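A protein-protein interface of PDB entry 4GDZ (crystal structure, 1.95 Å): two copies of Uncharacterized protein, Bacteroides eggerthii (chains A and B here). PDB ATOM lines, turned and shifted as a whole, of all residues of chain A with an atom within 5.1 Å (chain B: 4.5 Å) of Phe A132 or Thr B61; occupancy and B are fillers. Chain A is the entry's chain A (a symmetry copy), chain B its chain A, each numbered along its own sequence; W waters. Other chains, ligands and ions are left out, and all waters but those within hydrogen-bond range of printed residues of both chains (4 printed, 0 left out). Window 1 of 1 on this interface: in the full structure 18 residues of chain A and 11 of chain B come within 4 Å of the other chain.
Hydrophobic or aromatic side chains of chain B that line the printed part of chain A: Ala B62, Val B87, Tyr B88 and Pro B89.
Hydrophobic or aromatic side chains of chain A within 4 Å of the printed part of chain B: Phe A132.
Among the printed residues, 15 pairs touch across the chains.
Among the printed residues, no Asp or Glu carboxylate lies within 4 Å of a Lys or Arg side-chain nitrogen of the other chain.
Among the printed residues, pairs that only touch across the chains: Asn A117 with Ala B62 (3.3 Å), Thr A134 with Thr B61 (3.4 Å), Gln A130 with Pro B89 (3.4 Å), Phe A132 with Tyr B88 (3.5 Å), Val A144 with Gln B60 (3.5 Å), Phe A132 with Val B87 (3.6 Å), Ser A119 with Val B87 (3.7 Å), Phe A132 with Thr B61 (3.7 Å), Cys A118 with Val B87 (3.8 Å), Phe A132 with Pro B89 (3.8 Å) and Asn A117 with Val B87 (3.95 Å).
N of Val B54 is in hydrogen-bond range of O of Ala B62, at 2.9 Å.
The backbone carbonyl oxygen (O) of Cys A118 is in hydrogen-bond range of the backbone NH (N) of Leu A133.
N of Thr A145 sits at hydrogen-bond distance from O of Phe A132 (2.9 Å).
N of Thr A134 is in hydrogen-bond range of O of Thr A143 (2.9 Å).
Of the printed residues of chain B, Asn A117 touches Ala B62 (3.3 Å) and Val B87 (3.95 Å).
Of the printed residues of chain B, Cys A118 touches Val B87 (3.8 Å).
Phe A132 touches just these residues of chain B: Gln B60, Thr B61, Val B87, Tyr B88 and Pro B89.
Printed residues of chain B within 4 Å of Thr A134: Gln B60 and Thr B61.
Printed residues of chain B within 4 Å of Thr A143: Gln B60.
Thr B61 touches two residues of chain A.
Of the printed residues of chain A, Val B87 touches Asn A117 (3.95 Å), Cys A118 (3.8 Å), Ser A119 (3.7 Å) and Phe A132 (3.6 Å).
The nearest printed residue of chain B that does not touch Val A144 is Gly B59 (8.2 Å).
Water W1 lies within hydrogen-bond range of O of Val B87 (2.6 Å) and OG of Ser A119 (2.8 Å).
Water W3 lies within hydrogen-bond range of ND2 of Asn A117 (2.7 Å) and N of Val B87 (3.1 Å).
Water W2 lies within hydrogen-bond range of the side-chain hydroxyl of Thr A134 (2.8 Å), the side-chain hydroxyl of Thr B61 (2.8 Å) and the side-chain amide oxygen of Gln B60 (3.5 Å).
Water W4 lies within hydrogen-bond range of the side-chain hydroxyl of Thr B61 (2.9 Å) and the side-chain amide oxygen of Asn A117 (3.0 Å).
The side-chain amide nitrogen of Gln B60 sits at hydrogen-bond distance from the backbone carbonyl oxygen of Phe A132 (3.4 Å).
OE1 of Gln B60 is in hydrogen-bond range of OG1 of Thr A134 (2.9 Å).
The side-chain amide nitrogen (NE2) of Gln B60 is in hydrogen-bond range of the backbone carbonyl oxygen (O) of Thr A143 (3.3 Å).
OG1 of Thr A145 lies within hydrogen-bond range of NE2 of Gln B60, 3.1 Å away.
No position is printed for both chains.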
ATOM      1  N   ASN A 117      -3.316  20.206   1.526  1.00  0.00           N
ATOM      2  CA  ASN A 117      -3.436  19.184   0.470  1.00  0.00           C
ATOM      3  C   ASN A 117      -2.784  19.811  -0.767  1.00  0.00           C
ATOM      4  O   ASN A 117      -3.127  20.942  -1.129  1.00  0.00           O
ATOM      5  CB  ASN A 117      -4.907  18.924   0.150  1.00  0.00           C
ATOM      6  CG  ASN A 117      -5.672  18.216   1.264  1.00  0.00           C
ATOM      7  OD1 ASN A 117      -5.125  17.724   2.272  1.00  0.00           O
ATOM      8  ND2 ASN A 117      -6.961  18.165   1.087  1.00  0.00           N
ATOM      9  N   CYS A 118      -1.879  19.097  -1.418  1.00  0.00           N
ATOM     10  CA  CYS A 118      -1.112  19.608  -2.553  1.00  0.00           C
ATOM     11  C   CYS A 118      -0.957  18.545  -3.646  1.00  0.00           C
ATOM     12  O   CYS A 118      -0.771  17.382  -3.325  1.00  0.00           O
ATOM     13  CB  CYS A 118       0.277  20.025  -2.048  1.00  0.00           C
ATOM     14  SG  CYS A 118       1.440  20.629  -3.304  1.00  0.00           S
ATOM     15  N   SER A 119      -0.964  18.948  -4.909  1.00  0.00           N
ATOM     16  CA  SER A 119      -0.682  18.028  -6.013  1.00  0.00           C
ATOM     17  C   SER A 119       0.261  18.687  -6.977  1.00  0.00           C
ATOM     18  O   SER A 119       0.329  19.935  -7.069  1.00  0.00           O
ATOM     19  CB  SER A 119      -1.975  17.551  -6.732  1.00  0.00           C
ATOM     20  OG  SER A 119      -2.545  18.558  -7.552  1.00  0.00           O
ATOM     21  N   GLN A 130       2.254  11.608 -11.289  1.00  0.00           N
ATOM     22  CA  GLN A 130       1.379  12.544 -10.582  1.00  0.00           C
ATOM     23  C   GLN A 130       1.430  12.279  -9.068  1.00  0.00           C
ATOM     24  O   GLN A 130       1.358  11.134  -8.611  1.00  0.00           O
ATOM     25  CB  GLN A 130      -0.039  12.431 -11.112  1.00  0.00           C
ATOM     26  CG  GLN A 130      -0.955  13.472 -10.488  1.00  0.00           C
ATOM     27  CD  GLN A 130      -2.238  13.541 -11.250  1.00  0.00           C
ATOM     28  OE1 GLN A 130      -2.990  12.569 -11.285  1.00  0.00           O
ATOM     29  NE2 GLN A 130      -2.476  14.668 -11.892  1.00  0.00           N
ATOM     30  N   ILE A 131       1.613  13.351  -8.309  1.00  0.00           N
ATOM     31  CA  ILE A 131       1.911  13.305  -6.874  1.00  0.00           C
ATOM     32  C   ILE A 131       0.798  14.026  -6.098  1.00  0.00           C
ATOM     33  O   ILE A 131       0.430  15.137  -6.470  1.00  0.00           O
ATOM     34  CB  ILE A 131       3.234  14.049  -6.565  1.00  0.00           C
ATOM     35  CG1 ILE A 131       4.361  13.659  -7.559  1.00  0.00           C
ATOM     36  CG2 ILE A 131       3.635  13.817  -5.110  1.00  0.00           C
ATOM     37  CD1 ILE A 131       4.779  12.207  -7.526  1.00  0.00           C
ATOM     38  N   PHE A 132       0.310  13.423  -5.029  1.00  0.00           N
ATOM     39  CA  PHE A 132      -0.640  14.053  -4.110  1.00  0.00           C
ATOM     40  C   PHE A 132      -0.062  13.932  -2.708  1.00  0.00           C
ATOM     41  O   PHE A 132       0.254  12.848  -2.254  1.00  0.00           O
ATOM     42  CB  PHE A 132      -2.019  13.393  -4.187  1.00  0.00           C
ATOM     43  CG  PHE A 132      -3.039  13.962  -3.202  1.00  0.00           C
ATOM     44  CD1 PHE A 132      -3.459  15.295  -3.289  1.00  0.00           C
ATOM     45  CD2 PHE A 132      -3.507  13.200  -2.148  1.00  0.00           C
ATOM     46  CE1 PHE A 132      -4.353  15.835  -2.380  1.00  0.00           C
ATOM     47  CE2 PHE A 132      -4.423  13.726  -1.251  1.00  0.00           C
ATOM     48  CZ  PHE A 132      -4.842  15.051  -1.361  1.00  0.00           C
ATOM     49  N   LEU A 133       0.063  15.057  -2.026  1.00  0.00           N
ATOM     50  CA  LEU A 133       0.731  15.135  -0.727  1.00  0.00           C
ATOM     51  C   LEU A 133      -0.182  15.829   0.267  1.00  0.00           C
ATOM     52  O   LEU A 133      -0.785  16.865  -0.045  1.00  0.00           O
ATOM     53  CB  LEU A 133       2.058  15.894  -0.905  1.00  0.00           C
ATOM     54  CG  LEU A 133       2.978  16.241   0.268  1.00  0.00           C
ATOM     55  CD1 LEU A 133       4.299  16.744  -0.292  1.00  0.00           C
ATOM     56  CD2 LEU A 133       2.353  17.308   1.147  1.00  0.00           C
ATOM     57  N   THR A 134      -0.282  15.264   1.477  1.00  0.00           N
ATOM     58  CA  THR A 134      -1.103  15.827   2.533  1.00  0.00           C
ATOM     59  C   THR A 134      -0.253  15.977   3.794  1.00  0.00           C
ATOM     60  O   THR A 134       0.590  15.129   4.091  1.00  0.00           O
ATOM     61  CB  THR A 134      -2.333  14.962   2.859  1.00  0.00           C
ATOM     62  OG1 THR A 134      -1.878  13.661   3.261  1.00  0.00           O
ATOM     63  CG2 THR A 134      -3.263  14.873   1.642  1.00  0.00           C
ATOM     64  N   THR A 143       1.838  12.328   4.018  1.00  0.00           N
ATOM     65  CA  THR A 143       1.521  11.148   3.246  1.00  0.00           C
ATOM     66  C   THR A 143       1.507  11.538   1.783  1.00  0.00           C
ATOM     67  O   THR A 143       0.985  12.613   1.418  1.00  0.00           O
ATOM     68  CB  THR A 143       0.146  10.597   3.683  1.00  0.00           C
ATOM     69  OG1 THR A 143       0.236  10.324   5.089  1.00  0.00           O
ATOM     70  CG2 THR A 143      -0.242   9.320   2.910  1.00  0.00           C
ATOM     71  N   VAL A 144       2.094  10.696   0.945  1.00  0.00           N
ATOM     72  CA  VAL A 144       2.198  11.006  -0.467  1.00  0.00           C
ATOM     73  C   VAL A 144       1.692   9.809  -1.263  1.00  0.00           C
ATOM     74  O   VAL A 144       2.003   8.669  -0.924  1.00  0.00           O
ATOM     75  CB  VAL A 144       3.661  11.409  -0.828  1.00  0.00           C
ATOM     76  CG1 VAL A 144       4.663  10.244  -0.651  1.00  0.00           C
ATOM     77  CG2 VAL A 144       3.748  11.906  -2.248  1.00  0.00           C
ATOM     78  N   THR A 145       0.929  10.075  -2.323  1.00  0.00           N
ATOM     79  CA  THR A 145       0.562   9.076  -3.320  1.00  0.00           C
ATOM     80  C   THR A 145       1.205   9.419  -4.630  1.00  0.00           C
ATOM     81  O   THR A 145       1.119  10.576  -5.098  1.00  0.00           O
ATOM     82  CB  THR A 145      -0.993   9.046  -3.473  1.00  0.00           C
ATOM     83  OG1 THR A 145      -1.532   8.721  -2.185  1.00  0.00           O
ATOM     84  CG2 THR A 145      -1.483   7.997  -4.546  1.00  0.00           C
ATOM     85  N   GLN B  53     -13.503  15.669   6.797  1.00  0.00           N
ATOM     86  CA  GLN B  53     -12.662  15.085   5.795  1.00  0.00           C
ATOM     87  C   GLN B  53     -13.291  13.930   5.094  1.00  0.00           C
ATOM     88  O   GLN B  53     -14.154  13.236   5.640  1.00  0.00           O
ATOM     89  CB  GLN B  53     -11.288  14.670   6.366  1.00  0.00           C
ATOM     90  CG  GLN B  53     -11.337  13.669   7.456  1.00  0.00           C
ATOM     91  CD  GLN B  53      -9.966  13.137   7.891  1.00  0.00           C
ATOM     92  OE1 GLN B  53      -8.937  13.814   7.822  1.00  0.00           O
ATOM     93  NE2 GLN B  53      -9.972  11.911   8.380  1.00  0.00           N
ATOM     94  N   VAL B  54     -12.795  13.718   3.881  1.00  0.00           N
ATOM     95  CA  VAL B  54     -13.084  12.554   3.092  1.00  0.00           C
ATOM     96  C   VAL B  54     -11.861  11.644   3.147  1.00  0.00           C
ATOM     97  O   VAL B  54     -10.694  12.101   3.145  1.00  0.00           O
ATOM     98  CB  VAL B  54     -13.530  12.925   1.647  1.00  0.00           C
ATOM     99  CG1 VAL B  54     -12.500  13.798   0.956  1.00  0.00           C
ATOM    100  CG2 VAL B  54     -13.787  11.654   0.842  1.00  0.00           C
ATOM    101  N   MET B  55     -12.135  10.346   3.260  1.00  0.00           N
ATOM    102  CA  MET B  55     -11.116   9.337   3.375  1.00  0.00           C
ATOM    103  C   MET B  55     -11.049   8.459   2.135  1.00  0.00           C
ATOM    104  O   MET B  55     -12.072   7.974   1.647  1.00  0.00           O
ATOM    105  CB  MET B  55     -11.395   8.492   4.619  1.00  0.00           C
ATOM    106  CG  MET B  55     -11.430   9.356   5.905  1.00  0.00           C
ATOM    107  SD  MET B  55     -12.226   8.377   7.421  1.00  0.00           S
ATOM    108  CE  MET B  55     -11.265   6.624   7.264  1.00  0.00           C
ATOM    109  N   PHE B  56      -9.831   8.268   1.619  1.00  0.00           N
ATOM    110  CA  PHE B  56      -9.604   7.486   0.398  1.00  0.00           C
ATOM    111  C   PHE B  56      -9.106   6.077   0.724  1.00  0.00           C
ATOM    112  O   PHE B  56      -8.468   5.852   1.742  1.00  0.00           O
ATOM    113  CB  PHE B  56      -8.615   8.230  -0.548  1.00  0.00           C
ATOM    114  CG  PHE B  56      -9.104   9.600  -0.931  1.00  0.00           C
ATOM    115  CD1 PHE B  56     -10.046   9.763  -1.942  1.00  0.00           C
ATOM    116  CD2 PHE B  56      -8.724  10.709  -0.203  1.00  0.00           C
ATOM    117  CE1 PHE B  56     -10.555  11.015  -2.245  1.00  0.00           C
ATOM    118  CE2 PHE B  56      -9.214  11.953  -0.503  1.00  0.00           C
ATOM    119  CZ  PHE B  56     -10.143  12.118  -1.516  1.00  0.00           C
ATOM    120  N   GLY B  59      -5.563   5.198   1.951  1.00  0.00           N
ATOM    121  CA  GLY B  59      -5.124   5.691   3.282  1.00  0.00           C
ATOM    122  C   GLY B  59      -4.997   7.222   3.302  1.00  0.00           C
ATOM    123  O   GLY B  59      -4.801   7.824   4.354  1.00  0.00           O
ATOM    124  N   GLN B  60      -5.094   7.860   2.138  1.00  0.00           N
ATOM    125  CA  GLN B  60      -5.068   9.346   2.043  1.00  0.00           C
ATOM    126  C   GLN B  60      -6.344   9.965   2.601  1.00  0.00           C
ATOM    127  O   GLN B  60      -7.342   9.287   2.775  1.00  0.00           O
ATOM    128  CB  GLN B  60      -4.880   9.812   0.587  1.00  0.00           C
ATOM    129  CG  GLN B  60      -3.459   9.723   0.062  1.00  0.00           C
ATOM    130  CD  GLN B  60      -2.569  10.835   0.557  1.00  0.00           C
ATOM    131  OE1 GLN B  60      -2.906  11.569   1.495  1.00  0.00           O
ATOM    132  NE2 GLN B  60      -1.427  10.957  -0.054  1.00  0.00           N
ATOM    133  N   THR B  61      -6.300  11.259   2.886  1.00  0.00           N
ATOM    134  CA  THR B  61      -7.498  12.017   3.229  1.00  0.00           C
ATOM    135  C   THR B  61      -7.440  13.355   2.466  1.00  0.00           C
ATOM    136  O   THR B  61      -6.406  13.709   1.919  1.00  0.00           O
ATOM    137  CB  THR B  61      -7.547  12.364   4.716  1.00  0.00           C
ATOM    138  OG1 THR B  61      -6.426  13.183   4.983  1.00  0.00           O
ATOM    139  CG2 THR B  61      -7.493  11.099   5.633  1.00  0.00           C
ATOM    140  N   ALA B  62      -8.566  14.062   2.386  1.00  0.00           N
ATOM    141  CA  ALA B  62      -8.594  15.473   1.965  1.00  0.00           C
ATOM    142  C   ALA B  62      -9.625  16.161   2.826  1.00  0.00           C
ATOM    143  O   ALA B  62     -10.633  15.536   3.210  1.00  0.00           O
ATOM    144  CB  ALA B  62      -8.980  15.606   0.490  1.00  0.00           C
ATOM    145  N   VAL B  87      -8.294  18.598  -3.895  1.00  0.00           N
ATOM    146  CA  VAL B  87      -7.033  18.598  -4.621  1.00  0.00           C
ATOM    147  C   VAL B  87      -6.578  17.129  -4.934  1.00  0.00           C
ATOM    148  O   VAL B  87      -5.637  16.922  -5.710  1.00  0.00           O
ATOM    149  CB  VAL B  87      -5.989  19.442  -3.855  1.00  0.00           C
ATOM    150  CG1 VAL B  87      -4.571  19.283  -4.415  1.00  0.00           C
ATOM    151  CG2 VAL B  87      -6.382  20.937  -3.917  1.00  0.00           C
ATOM    152  N   TYR B  88      -7.247  16.130  -4.351  1.00  0.00           N
ATOM    153  CA  TYR B  88      -6.941  14.726  -4.700  1.00  0.00           C
ATOM    154  C   TYR B  88      -7.228  14.572  -6.229  1.00  0.00           C
ATOM    155  O   TYR B  88      -8.331  14.810  -6.655  1.00  0.00           O
ATOM    156  CB  TYR B  88      -7.759  13.792  -3.846  1.00  0.00           C
ATOM    157  CG  TYR B  88      -7.465  12.323  -4.029  1.00  0.00           C
ATOM    158  CD1 TYR B  88      -7.921  11.636  -5.160  1.00  0.00           C
ATOM    159  CD2 TYR B  88      -6.756  11.610  -3.079  1.00  0.00           C
ATOM    160  CE1 TYR B  88      -7.645  10.280  -5.349  1.00  0.00           C
ATOM    161  CE2 TYR B  88      -6.504  10.253  -3.243  1.00  0.00           C
ATOM    162  CZ  TYR B  88      -6.945   9.591  -4.373  1.00  0.00           C
ATOM    163  OH  TYR B  88      -6.689   8.246  -4.540  1.00  0.00           O
ATOM    164  N   PRO B  89      -6.199  14.284  -7.038  1.00  0.00           N
ATOM    165  CA  PRO B  89      -6.385  14.413  -8.491  1.00  0.00           C
ATOM    166  C   PRO B  89      -7.320  13.335  -9.042  1.00  0.00           C
ATOM    167  O   PRO B  89      -7.377  12.218  -8.498  1.00  0.00           O
ATOM    168  CB  PRO B  89      -4.996  14.201  -9.050  1.00  0.00           C
ATOM    169  CG  PRO B  89      -4.062  14.344  -7.915  1.00  0.00           C
ATOM    170  CD  PRO B  89      -4.809  13.942  -6.697  1.00  0.00           C
HETATM  171  O   HOH W   1      -5.250  18.195  -7.978  1.00  0.00           O
HETATM  172  O   HOH W   2      -3.775  12.281   4.783  1.00  0.00           O
HETATM  173  O   HOH W   3      -8.308  19.425  -0.923  1.00  0.00           O
HETATM  174  O   HOH W   4      -6.358  16.054   4.444  1.00  0.00           O
